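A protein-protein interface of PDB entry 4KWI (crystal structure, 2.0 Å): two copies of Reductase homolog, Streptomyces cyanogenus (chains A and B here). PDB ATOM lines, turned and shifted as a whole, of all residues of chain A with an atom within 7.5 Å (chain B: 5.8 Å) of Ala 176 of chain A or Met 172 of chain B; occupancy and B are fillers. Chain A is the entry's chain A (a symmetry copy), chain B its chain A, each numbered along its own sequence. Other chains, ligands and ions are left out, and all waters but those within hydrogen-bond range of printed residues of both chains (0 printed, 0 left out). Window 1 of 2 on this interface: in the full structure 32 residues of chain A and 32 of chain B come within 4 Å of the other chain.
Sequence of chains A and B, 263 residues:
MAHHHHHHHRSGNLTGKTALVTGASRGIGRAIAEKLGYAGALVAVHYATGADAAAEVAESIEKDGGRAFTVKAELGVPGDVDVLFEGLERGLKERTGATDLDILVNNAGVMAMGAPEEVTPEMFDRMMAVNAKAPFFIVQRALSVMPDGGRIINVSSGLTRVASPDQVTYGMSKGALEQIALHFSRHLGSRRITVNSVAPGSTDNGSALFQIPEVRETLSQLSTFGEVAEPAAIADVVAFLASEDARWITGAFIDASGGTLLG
CE of Met 172 of chain B touches O of Ala 132 of chain A, at 3.4 Å. Lys 133 of chain A touches Phe 124 of chain B. CZ of Phe 136 of chain A touches CG2 of Thr 169 of chain B (3.9 Å). CD1 of Phe 136 of chain A touches SD of Met 172 of chain B, at 3.9 Å. Met 172 of chain A touches Ala 176 of chain B. CG of Gln 179 of chain A touches O of Gly 171 of chain B, at 3.3 Å. CG1 of Ile 180 of chain A touches SD of Met 172 of chain B, 3.8 Å away. His 183 of chain A touches Val 168 of chain B. His 183 of chain A touches Gly 171 of chain B. Val 168 of chain B touches Phe 184 of chain A.
Of the 25 printed residues of chain A, 11 touch a printed residue of chain B. Of the 13 printed residues of chain B, 7 touch a printed residue of chain A.
Of the printed residues of chain B, Ala 176 of chain A touches Met 172. Gly 171 of chain B touches just these residues of chain A: Gln 179 (3.3 Å) and His 183 (3.96 Å). Printed residues of chain A within 4 Å of Thr 169 of chain B: Phe 136. Of the printed residues of chain A, Met 128 of chain B touches Met 128 (3.6 Å). Of the printed residues of chain A, Val 168 of chain B touches Phe 136 (3.8 Å), His 183 (3.8 Å) and Phe 184 (3.8 Å). Of the printed residues of chain B, Ile 180 of chain A touches Met 172 (3.8 Å). Ser 156 of chain A touches none of the printed residues of chain B. The nearest printed residue of chain B that does not touch Ala 176 of chain A is Ala 176 of chain B (4.01 Å).
O of Met 128 of chain A sits at hydrogen-bond distance from N of Lys 133 of chain A, 3.1 Å away. The side-chain amide oxygen (OE1) of Gln 179 of chain A lies within hydrogen-bond range of a ring nitrogen (NE2) of His 183 of chain A.
Met 128 of chain A touches its own counterpart, Met 128 of chain B. Met 172 of chain A touches Ala 176 of chain B, and with the chains exchanged Ala 176 of chain A touches Met 172 of chain B. Positions printed for both chains: 128, 170, 171, 172, 173, 174, 175, 176 and 177.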
ATOM      1  N   MET A 128     -11.761 -15.530   9.936  1.00  0.00           N
ATOM      2  CA  MET A 128     -11.772 -16.419   8.771  1.00  0.00           C
ATOM      3  C   MET A 128     -10.419 -16.437   8.044  1.00  0.00           C
ATOM      4  O   MET A 128      -9.954 -17.495   7.653  1.00  0.00           O
ATOM      5  CB  MET A 128     -12.901 -16.014   7.831  1.00  0.00           C
ATOM      6  CG  MET A 128     -13.486 -17.122   6.978  1.00  0.00           C
ATOM      7  SD  MET A 128     -13.883 -18.691   7.791  1.00  0.00           S
ATOM      8  CE  MET A 128     -15.290 -18.237   8.805  1.00  0.00           C
ATOM      9  N   ASN A 131      -7.849 -18.492  10.469  1.00  0.00           N
ATOM     10  CA  ASN A 131      -8.231 -19.867  10.867  1.00  0.00           C
ATOM     11  C   ASN A 131      -8.673 -20.822   9.741  1.00  0.00           C
ATOM     12  O   ASN A 131      -8.594 -22.040   9.906  1.00  0.00           O
ATOM     13  CB  ASN A 131      -9.281 -19.847  11.972  1.00  0.00           C
ATOM     14  CG  ASN A 131      -8.793 -19.160  13.240  1.00  0.00           C
ATOM     15  OD1 ASN A 131      -7.633 -18.749  13.337  1.00  0.00           O
ATOM     16  ND2 ASN A 131      -9.679 -19.033  14.220  1.00  0.00           N
ATOM     17  N   ALA A 132      -9.118 -20.288   8.605  1.00  0.00           N
ATOM     18  CA  ALA A 132      -9.615 -21.155   7.513  1.00  0.00           C
ATOM     19  C   ALA A 132      -8.941 -20.962   6.164  1.00  0.00           C
ATOM     20  O   ALA A 132      -8.574 -21.937   5.510  1.00  0.00           O
ATOM     21  CB  ALA A 132     -11.132 -21.023   7.365  1.00  0.00           C
ATOM     22  N   LYS A 133      -8.824 -19.703   5.741  1.00  0.00           N
ATOM     23  CA  LYS A 133      -8.261 -19.356   4.449  1.00  0.00           C
ATOM     24  C   LYS A 133      -6.779 -19.707   4.384  1.00  0.00           C
ATOM     25  O   LYS A 133      -6.334 -20.405   3.466  1.00  0.00           O
ATOM     26  CB  LYS A 133      -8.485 -17.859   4.176  1.00  0.00           C
ATOM     27  CG  LYS A 133      -8.102 -17.395   2.787  1.00  0.00           C
ATOM     28  CD  LYS A 133      -8.551 -15.950   2.523  1.00  0.00           C
ATOM     29  CE  LYS A 133      -7.843 -15.400   1.293  1.00  0.00           C
ATOM     30  NZ  LYS A 133      -7.918 -13.914   1.178  1.00  0.00           N
ATOM     31  N   ALA A 134      -6.008 -19.220   5.345  1.00  0.00           N
ATOM     32  CA  ALA A 134      -4.579 -19.495   5.353  1.00  0.00           C
ATOM     33  C   ALA A 134      -4.320 -21.013   5.403  1.00  0.00           C
ATOM     34  O   ALA A 134      -3.544 -21.527   4.577  1.00  0.00           O
ATOM     35  CB  ALA A 134      -3.869 -18.760   6.484  1.00  0.00           C
ATOM     36  N   PRO A 135      -4.988 -21.741   6.327  1.00  0.00           N
ATOM     37  CA  PRO A 135      -4.758 -23.183   6.269  1.00  0.00           C
ATOM     38  C   PRO A 135      -5.058 -23.834   4.901  1.00  0.00           C
ATOM     39  O   PRO A 135      -4.346 -24.766   4.514  1.00  0.00           O
ATOM     40  CB  PRO A 135      -5.673 -23.729   7.372  1.00  0.00           C
ATOM     41  CG  PRO A 135      -5.657 -22.644   8.407  1.00  0.00           C
ATOM     42  CD  PRO A 135      -5.628 -21.352   7.605  1.00  0.00           C
ATOM     43  N   PHE A 136      -6.084 -23.352   4.192  1.00  0.00           N
ATOM     44  CA  PHE A 136      -6.417 -23.899   2.875  1.00  0.00           C
ATOM     45  C   PHE A 136      -5.305 -23.622   1.856  1.00  0.00           C
ATOM     46  O   PHE A 136      -4.884 -24.524   1.143  1.00  0.00           O
ATOM     47  CB  PHE A 136      -7.772 -23.387   2.327  1.00  0.00           C
ATOM     48  CG  PHE A 136      -7.984 -23.739   0.875  1.00  0.00           C
ATOM     49  CD1 PHE A 136      -8.559 -24.951   0.515  1.00  0.00           C
ATOM     50  CD2 PHE A 136      -7.538 -22.888  -0.130  1.00  0.00           C
ATOM     51  CE1 PHE A 136      -8.707 -25.300  -0.819  1.00  0.00           C
ATOM     52  CE2 PHE A 136      -7.680 -23.226  -1.468  1.00  0.00           C
ATOM     53  CZ  PHE A 136      -8.270 -24.437  -1.816  1.00  0.00           C
ATOM     54  N   PHE A 137      -4.845 -22.375   1.773  1.00  0.00           N
ATOM     55  CA  PHE A 137      -3.776 -22.022   0.852  1.00  0.00           C
ATOM     56  C   PHE A 137      -2.418 -22.617   1.262  1.00  0.00           C
ATOM     57  O   PHE A 137      -1.590 -22.915   0.398  1.00  0.00           O
ATOM     58  CB  PHE A 137      -3.753 -20.503   0.560  1.00  0.00           C
ATOM     59  CG  PHE A 137      -4.930 -20.056  -0.268  1.00  0.00           C
ATOM     60  CD1 PHE A 137      -4.977 -20.323  -1.632  1.00  0.00           C
ATOM     61  CD2 PHE A 137      -6.023 -19.439   0.326  1.00  0.00           C
ATOM     62  CE1 PHE A 137      -6.078 -19.956  -2.390  1.00  0.00           C
ATOM     63  CE2 PHE A 137      -7.132 -19.073  -0.421  1.00  0.00           C
ATOM     64  CZ  PHE A 137      -7.162 -19.342  -1.782  1.00  0.00           C
ATOM     65  N   ASN A 154      -4.851 -30.747  10.931  1.00  0.00           N
ATOM     66  CA  ASN A 154      -5.443 -29.451  11.185  1.00  0.00           C
ATOM     67  C   ASN A 154      -5.997 -29.385  12.612  1.00  0.00           C
ATOM     68  O   ASN A 154      -6.849 -30.189  13.024  1.00  0.00           O
ATOM     69  CB  ASN A 154      -6.502 -29.109  10.106  1.00  0.00           C
ATOM     70  CG  ASN A 154      -5.945 -29.229   8.672  1.00  0.00           C
ATOM     71  OD1 ASN A 154      -4.804 -28.814   8.386  1.00  0.00           O
ATOM     72  ND2 ASN A 154      -6.744 -29.772   7.772  1.00  0.00           N
ATOM     73  N   SER A 156      -8.313 -28.178  15.170  1.00  0.00           N
ATOM     74  CA  SER A 156      -9.637 -27.588  15.275  1.00  0.00           C
ATOM     75  C   SER A 156      -9.945 -27.177  16.724  1.00  0.00           C
ATOM     76  O   SER A 156      -9.095 -26.608  17.411  1.00  0.00           O
ATOM     77  CB  SER A 156     -10.683 -28.575  14.775  1.00  0.00           C
ATOM     78  OG  SER A 156     -11.902 -27.913  14.510  1.00  0.00           O
ATOM     79  N   THR A 160     -16.608 -26.702  17.808  1.00  0.00           N
ATOM     80  CA  THR A 160     -17.401 -27.009  16.621  1.00  0.00           C
ATOM     81  C   THR A 160     -18.541 -27.994  16.931  1.00  0.00           C
ATOM     82  O   THR A 160     -19.356 -28.306  16.058  1.00  0.00           O
ATOM     83  CB  THR A 160     -16.534 -27.527  15.454  1.00  0.00           C
ATOM     84  OG1 THR A 160     -15.881 -28.734  15.850  1.00  0.00           O
ATOM     85  CG2 THR A 160     -15.485 -26.489  15.057  1.00  0.00           C
ATOM     86  N   TYR A 170     -15.556 -17.782  15.835  1.00  0.00           N
ATOM     87  CA  TYR A 170     -14.503 -18.776  16.031  1.00  0.00           C
ATOM     88  C   TYR A 170     -14.982 -20.164  15.570  1.00  0.00           C
ATOM     89  O   TYR A 170     -14.303 -20.831  14.782  1.00  0.00           O
ATOM     90  CB  TYR A 170     -14.074 -18.811  17.484  1.00  0.00           C
ATOM     91  CG  TYR A 170     -13.018 -19.851  17.781  1.00  0.00           C
ATOM     92  CD1 TYR A 170     -11.662 -19.549  17.651  1.00  0.00           C
ATOM     93  CD2 TYR A 170     -13.374 -21.128  18.218  1.00  0.00           C
ATOM     94  CE1 TYR A 170     -10.689 -20.502  17.934  1.00  0.00           C
ATOM     95  CE2 TYR A 170     -12.408 -22.082  18.505  1.00  0.00           C
ATOM     96  CZ  TYR A 170     -11.070 -21.766  18.360  1.00  0.00           C
ATOM     97  OH  TYR A 170     -10.099 -22.705  18.649  1.00  0.00           O
ATOM     98  N   GLY A 171     -16.154 -20.578  16.059  1.00  0.00           N
ATOM     99  CA  GLY A 171     -16.801 -21.826  15.636  1.00  0.00           C
ATOM    100  C   GLY A 171     -16.936 -21.946  14.127  1.00  0.00           C
ATOM    101  O   GLY A 171     -16.529 -22.951  13.551  1.00  0.00           O
ATOM    102  N   MET A 172     -17.501 -20.915  13.484  1.00  0.00           N
ATOM    103  CA  MET A 172     -17.626 -20.910  12.025  1.00  0.00           C
ATOM    104  C   MET A 172     -16.291 -21.171  11.306  1.00  0.00           C
ATOM    105  O   MET A 172     -16.242 -21.987  10.385  1.00  0.00           O
ATOM    106  CB  MET A 172     -18.270 -19.606  11.512  1.00  0.00           C
ATOM    107  CG  MET A 172     -19.734 -19.416  11.903  1.00  0.00           C
ATOM    108  SD  MET A 172     -20.430 -17.869  11.268  1.00  0.00           S
ATOM    109  CE  MET A 172     -20.455 -18.205   9.495  1.00  0.00           C
ATOM    110  N   SER A 173     -15.224 -20.483  11.726  1.00  0.00           N
ATOM    111  CA  SER A 173     -13.910 -20.636  11.116  1.00  0.00           C
ATOM    112  C   SER A 173     -13.384 -22.063  11.238  1.00  0.00           C
ATOM    113  O   SER A 173     -12.840 -22.622  10.274  1.00  0.00           O
ATOM    114  CB  SER A 173     -12.895 -19.606  11.645  1.00  0.00           C
ATOM    115  OG  SER A 173     -12.504 -19.822  12.985  1.00  0.00           O
ATOM    116  N   LYS A 174     -13.595 -22.659  12.404  1.00  0.00           N
ATOM    117  CA  LYS A 174     -13.123 -24.016  12.664  1.00  0.00           C
ATOM    118  C   LYS A 174     -13.970 -25.054  11.945  1.00  0.00           C
ATOM    119  O   LYS A 174     -13.462 -26.102  11.550  1.00  0.00           O
ATOM    120  CB  LYS A 174     -13.020 -24.287  14.166  1.00  0.00           C
ATOM    121  CG  LYS A 174     -11.953 -23.456  14.872  1.00  0.00           C
ATOM    122  CD  LYS A 174     -10.544 -23.843  14.438  1.00  0.00           C
ATOM    123  CE  LYS A 174      -9.506 -23.208  15.349  1.00  0.00           C
ATOM    124  NZ  LYS A 174      -8.123 -23.662  15.033  1.00  0.00           N
ATOM    125  N   GLY A 175     -15.246 -24.742  11.714  1.00  0.00           N
ATOM    126  CA  GLY A 175     -16.089 -25.625  10.923  1.00  0.00           C
ATOM    127  C   GLY A 175     -15.639 -25.651   9.463  1.00  0.00           C
ATOM    128  O   GLY A 175     -15.686 -26.692   8.828  1.00  0.00           O
ATOM    129  N   ALA A 176     -15.219 -24.493   8.935  1.00  0.00           N
ATOM    130  CA  ALA A 176     -14.588 -24.416   7.614  1.00  0.00           C
ATOM    131  C   ALA A 176     -13.283 -25.212   7.562  1.00  0.00           C
ATOM    132  O   ALA A 176     -13.032 -25.968   6.599  1.00  0.00           O
ATOM    133  CB  ALA A 176     -14.349 -22.961   7.207  1.00  0.00           C
ATOM    134  N   LEU A 177     -12.468 -25.052   8.601  1.00  0.00           N
ATOM    135  CA  LEU A 177     -11.196 -25.799   8.730  1.00  0.00           C
ATOM    136  C   LEU A 177     -11.434 -27.308   8.655  1.00  0.00           C
ATOM    137  O   LEU A 177     -10.796 -28.003   7.863  1.00  0.00           O
ATOM    138  CB  LEU A 177     -10.449 -25.445  10.024  1.00  0.00           C
ATOM    139  CG  LEU A 177      -9.102 -26.177  10.234  1.00  0.00           C
ATOM    140  CD1 LEU A 177      -7.972 -25.506   9.475  1.00  0.00           C
ATOM    141  CD2 LEU A 177      -8.742 -26.249  11.696  1.00  0.00           C
ATOM    142  N   GLU A 178     -12.397 -27.798   9.424  1.00  0.00           N
ATOM    143  CA  GLU A 178     -12.688 -29.238   9.430  1.00  0.00           C
ATOM    144  C   GLU A 178     -13.047 -29.824   8.053  1.00  0.00           C
ATOM    145  O   GLU A 178     -12.783 -30.992   7.797  1.00  0.00           O
ATOM    146  CB  GLU A 178     -13.735 -29.584  10.500  1.00  0.00           C
ATOM    147  CG  GLU A 178     -13.197 -29.361  11.907  1.00  0.00           C
ATOM    148  CD  GLU A 178     -14.180 -29.647  13.029  1.00  0.00           C
ATOM    149  OE1 GLU A 178     -15.221 -30.288  12.802  1.00  0.00           O
ATOM    150  OE2 GLU A 178     -13.893 -29.231  14.169  1.00  0.00           O
ATOM    151  N   GLN A 179     -13.619 -29.015   7.162  1.00  0.00           N
ATOM    152  CA  GLN A 179     -13.905 -29.469   5.791  1.00  0.00           C
ATOM    153  C   GLN A 179     -12.649 -29.786   4.979  1.00  0.00           C
ATOM    154  O   GLN A 179     -12.702 -30.521   3.983  1.00  0.00           O
ATOM    155  CB  GLN A 179     -14.754 -28.434   5.042  1.00  0.00           C
ATOM    156  CG  GLN A 179     -16.203 -28.342   5.501  1.00  0.00           C
ATOM    157  CD  GLN A 179     -17.005 -29.570   5.132  1.00  0.00           C
ATOM    158  OE1 GLN A 179     -17.098 -29.954   3.943  1.00  0.00           O
ATOM    159  NE2 GLN A 179     -17.570 -30.221   6.142  1.00  0.00           N
ATOM    160  N   ILE A 180     -11.507 -29.237   5.372  1.00  0.00           N
ATOM    161  CA  ILE A 180     -10.278 -29.555   4.649  1.00  0.00           C
ATOM    162  C   ILE A 180      -9.977 -31.064   4.703  1.00  0.00           C
ATOM    163  O   ILE A 180      -9.720 -31.702   3.658  1.00  0.00           O
ATOM    164  CB  ILE A 180      -9.070 -28.696   5.106  1.00  0.00           C
ATOM    165  CG1 ILE A 180      -9.283 -27.229   4.688  1.00  0.00           C
ATOM    166  CG2 ILE A 180      -7.770 -29.246   4.503  1.00  0.00           C
ATOM    167  CD1 ILE A 180      -8.346 -26.232   5.355  1.00  0.00           C
ATOM    168  N   ALA A 181     -10.021 -31.635   5.904  1.00  0.00           N
ATOM    169  CA  ALA A 181      -9.788 -33.071   6.073  1.00  0.00           C
ATOM    170  C   ALA A 181     -10.760 -33.901   5.233  1.00  0.00           C
ATOM    171  O   ALA A 181     -10.337 -34.805   4.512  1.00  0.00           O
ATOM    172  CB  ALA A 181      -9.843 -33.472   7.539  1.00  0.00           C
ATOM    173  N   HIS A 183     -12.483 -33.339   2.401  1.00  0.00           N
ATOM    174  CA  HIS A 183     -12.369 -33.300   0.947  1.00  0.00           C
ATOM    175  C   HIS A 183     -11.001 -33.632   0.406  1.00  0.00           C
ATOM    176  O   HIS A 183     -10.898 -34.326  -0.603  1.00  0.00           O
ATOM    177  CB  HIS A 183     -12.871 -31.952   0.398  1.00  0.00           C
ATOM    178  CG  HIS A 183     -14.327 -31.686   0.702  1.00  0.00           C
ATOM    179  ND1 HIS A 183     -15.320 -32.234  -0.003  1.00  0.00           N
ATOM    180  CD2 HIS A 183     -14.934 -30.904   1.697  1.00  0.00           C
ATOM    181  CE1 HIS A 183     -16.508 -31.835   0.496  1.00  0.00           C
ATOM    182  NE2 HIS A 183     -16.270 -31.030   1.547  1.00  0.00           N
ATOM    183  N   PHE A 184      -9.944 -33.144   1.054  1.00  0.00           N
ATOM    184  CA  PHE A 184      -8.567 -33.491   0.639  1.00  0.00           C
ATOM    185  C   PHE A 184      -8.163 -34.950   0.919  1.00  0.00           C
ATOM    186  O   PHE A 184      -7.275 -35.498   0.238  1.00  0.00           O
ATOM    187  CB  PHE A 184      -7.533 -32.524   1.233  1.00  0.00           C
ATOM    188  CG  PHE A 184      -7.381 -31.244   0.445  1.00  0.00           C
ATOM    189  CD1 PHE A 184      -6.565 -31.194  -0.684  1.00  0.00           C
ATOM    190  CD2 PHE A 184      -8.070 -30.088   0.823  1.00  0.00           C
ATOM    191  CE1 PHE A 184      -6.421 -30.007  -1.403  1.00  0.00           C
ATOM    192  CE2 PHE A 184      -7.933 -28.909   0.105  1.00  0.00           C
ATOM    193  CZ  PHE A 184      -7.107 -28.868  -1.013  1.00  0.00           C
ATOM    194  N   PHE B 124     -11.839 -17.885  -3.241  1.00  0.00           N
ATOM    195  CA  PHE B 124     -12.083 -18.266  -1.862  1.00  0.00           C
ATOM    196  C   PHE B 124     -12.858 -17.172  -1.100  1.00  0.00           C
ATOM    197  O   PHE B 124     -13.809 -17.479  -0.384  1.00  0.00           O
ATOM    198  CB  PHE B 124     -10.753 -18.596  -1.152  1.00  0.00           C
ATOM    199  CG  PHE B 124     -10.932 -19.157   0.230  1.00  0.00           C
ATOM    200  CD1 PHE B 124     -11.257 -18.317   1.306  1.00  0.00           C
ATOM    201  CD2 PHE B 124     -10.806 -20.524   0.462  1.00  0.00           C
ATOM    202  CE1 PHE B 124     -11.463 -18.836   2.575  1.00  0.00           C
ATOM    203  CE2 PHE B 124     -10.995 -21.042   1.731  1.00  0.00           C
ATOM    204  CZ  PHE B 124     -11.324 -20.200   2.794  1.00  0.00           C
ATOM    205  N   MET B 128     -16.648 -17.585   0.434  1.00  0.00           N
ATOM    206  CA  MET B 128     -16.876 -17.324   1.858  1.00  0.00           C
ATOM    207  C   MET B 128     -17.767 -16.094   2.085  1.00  0.00           C
ATOM    208  O   MET B 128     -18.650 -16.130   2.928  1.00  0.00           O
ATOM    209  CB  MET B 128     -15.538 -17.177   2.571  1.00  0.00           C
ATOM    210  CG  MET B 128     -15.520 -17.559   4.038  1.00  0.00           C
ATOM    211  SD  MET B 128     -16.313 -19.116   4.513  1.00  0.00           S
ATOM    212  CE  MET B 128     -15.196 -20.330   3.812  1.00  0.00           C
ATOM    213  N   GLN B 167     -15.113 -29.501  -4.969  1.00  0.00           N
ATOM    214  CA  GLN B 167     -16.070 -28.665  -4.253  1.00  0.00           C
ATOM    215  C   GLN B 167     -15.566 -28.224  -2.881  1.00  0.00           C
ATOM    216  O   GLN B 167     -16.361 -27.771  -2.041  1.00  0.00           O
ATOM    217  CB  GLN B 167     -17.394 -29.424  -4.072  1.00  0.00           C
ATOM    218  CG  GLN B 167     -18.064 -29.916  -5.354  1.00  0.00           C
ATOM    219  CD  GLN B 167     -18.813 -28.821  -6.090  1.00  0.00           C
ATOM    220  OE1 GLN B 167     -18.550 -27.634  -5.894  1.00  0.00           O
ATOM    221  NE2 GLN B 167     -19.758 -29.215  -6.940  1.00  0.00           N
ATOM    222  N   VAL B 168     -14.255 -28.337  -2.647  1.00  0.00           N
ATOM    223  CA  VAL B 168     -13.707 -28.122  -1.293  1.00  0.00           C
ATOM    224  C   VAL B 168     -13.994 -26.726  -0.687  1.00  0.00           C
ATOM    225  O   VAL B 168     -14.398 -26.636   0.462  1.00  0.00           O
ATOM    226  CB  VAL B 168     -12.216 -28.540  -1.170  1.00  0.00           C
ATOM    227  CG1 VAL B 168     -11.332 -27.780  -2.148  1.00  0.00           C
ATOM    228  CG2 VAL B 168     -11.722 -28.366   0.268  1.00  0.00           C
ATOM    229  N   THR B 169     -13.805 -25.651  -1.454  1.00  0.00           N
ATOM    230  CA  THR B 169     -14.097 -24.306  -0.933  1.00  0.00           C
ATOM    231  C   THR B 169     -15.599 -24.086  -0.735  1.00  0.00           C
ATOM    232  O   THR B 169     -16.024 -23.409   0.200  1.00  0.00           O
ATOM    233  CB  THR B 169     -13.511 -23.177  -1.816  1.00  0.00           C
ATOM    234  OG1 THR B 169     -14.112 -23.217  -3.114  1.00  0.00           O
ATOM    235  CG2 THR B 169     -11.989 -23.320  -1.949  1.00  0.00           C
ATOM    236  N   TYR B 170     -16.403 -24.654  -1.623  1.00  0.00           N
ATOM    237  CA  TYR B 170     -17.847 -24.685  -1.397  1.00  0.00           C
ATOM    238  C   TYR B 170     -18.167 -25.396  -0.071  1.00  0.00           C
ATOM    239  O   TYR B 170     -18.895 -24.856   0.769  1.00  0.00           O
ATOM    240  CB  TYR B 170     -18.548 -25.365  -2.556  1.00  0.00           C
ATOM    241  CG  TYR B 170     -20.044 -25.481  -2.376  1.00  0.00           C
ATOM    242  CD1 TYR B 170     -20.895 -24.457  -2.792  1.00  0.00           C
ATOM    243  CD2 TYR B 170     -20.611 -26.627  -1.816  1.00  0.00           C
ATOM    244  CE1 TYR B 170     -22.273 -24.567  -2.638  1.00  0.00           C
ATOM    245  CE2 TYR B 170     -21.986 -26.744  -1.660  1.00  0.00           C
ATOM    246  CZ  TYR B 170     -22.810 -25.714  -2.070  1.00  0.00           C
ATOM    247  OH  TYR B 170     -24.180 -25.821  -1.928  1.00  0.00           O
ATOM    248  N   GLY B 171     -17.610 -26.598   0.106  1.00  0.00           N
ATOM    249  CA  GLY B 171     -17.728 -27.357   1.356  1.00  0.00           C
ATOM    250  C   GLY B 171     -17.333 -26.553   2.583  1.00  0.00           C
ATOM    251  O   GLY B 171     -18.094 -26.479   3.542  1.00  0.00           O
ATOM    252  N   MET B 172     -16.141 -25.940   2.548  1.00  0.00           N
ATOM    253  CA  MET B 172     -15.693 -25.095   3.657  1.00  0.00           C
ATOM    254  C   MET B 172     -16.713 -24.006   4.036  1.00  0.00           C
ATOM    255  O   MET B 172     -17.004 -23.827   5.218  1.00  0.00           O
ATOM    256  CB  MET B 172     -14.313 -24.467   3.374  1.00  0.00           C
ATOM    257  CG  MET B 172     -13.155 -25.461   3.314  1.00  0.00           C
ATOM    258  SD  MET B 172     -11.564 -24.660   2.982  1.00  0.00           S
ATOM    259  CE  MET B 172     -11.317 -23.738   4.513  1.00  0.00           C
ATOM    260  N   SER B 173     -17.246 -23.293   3.038  1.00  0.00           N
ATOM    261  CA  SER B 173     -18.213 -22.230   3.272  1.00  0.00           C
ATOM    262  C   SER B 173     -19.479 -22.745   3.951  1.00  0.00           C
ATOM    263  O   SER B 173     -19.996 -22.117   4.886  1.00  0.00           O
ATOM    264  CB  SER B 173     -18.534 -21.436   1.992  1.00  0.00           C
ATOM    265  OG  SER B 173     -19.283 -22.162   1.040  1.00  0.00           O
ATOM    266  N   LYS B 174     -19.938 -23.908   3.510  1.00  0.00           N
ATOM    267  CA  LYS B 174     -21.154 -24.505   4.055  1.00  0.00           C
ATOM    268  C   LYS B 174     -20.924 -25.085   5.441  1.00  0.00           C
ATOM    269  O   LYS B 174     -21.832 -25.090   6.270  1.00  0.00           O
ATOM    270  CB  LYS B 174     -21.750 -25.528   3.086  1.00  0.00           C
ATOM    271  CG  LYS B 174     -22.268 -24.920   1.787  1.00  0.00           C
ATOM    272  CD  LYS B 174     -23.487 -24.032   2.015  1.00  0.00           C
ATOM    273  CE  LYS B 174     -24.146 -23.672   0.693  1.00  0.00           C
ATOM    274  NZ  LYS B 174     -25.411 -22.909   0.882  1.00  0.00           N
ATOM    275  N   GLY B 175     -19.693 -25.517   5.722  1.00  0.00           N
ATOM    276  CA  GLY B 175     -19.359 -25.970   7.063  1.00  0.00           C
ATOM    277  C   GLY B 175     -19.376 -24.808   8.054  1.00  0.00           C
ATOM    278  O   GLY B 175     -19.791 -24.979   9.189  1.00  0.00           O
ATOM    279  N   ALA B 176     -18.907 -23.631   7.620  1.00  0.00           N
ATOM    280  CA  ALA B 176     -19.038 -22.397   8.401  1.00  0.00           C
ATOM    281  C   ALA B 176     -20.504 -22.023   8.627  1.00  0.00           C
ATOM    282  O   ALA B 176     -20.907 -21.668   9.755  1.00  0.00           O
ATOM    283  CB  ALA B 176     -18.285 -21.245   7.733  1.00  0.00           C
ATOM    284  N   LEU B 177     -21.295 -22.119   7.562  1.00  0.00           N
ATOM    285  CA  LEU B 177     -22.749 -21.852   7.630  1.00  0.00           C
ATOM    286  C   LEU B 177     -23.420 -22.728   8.689  1.00  0.00           C
ATOM    287  O   LEU B 177     -24.131 -22.225   9.559  1.00  0.00           O
ATOM    288  CB  LEU B 177     -23.436 -22.045   6.271  1.00  0.00           C
ATOM    289  CG  LEU B 177     -24.959 -21.778   6.252  1.00  0.00           C
ATOM    290  CD1 LEU B 177     -25.271 -20.298   6.124  1.00  0.00           C
ATOM    291  CD2 LEU B 177     -25.631 -22.524   5.127  1.00  0.00           C
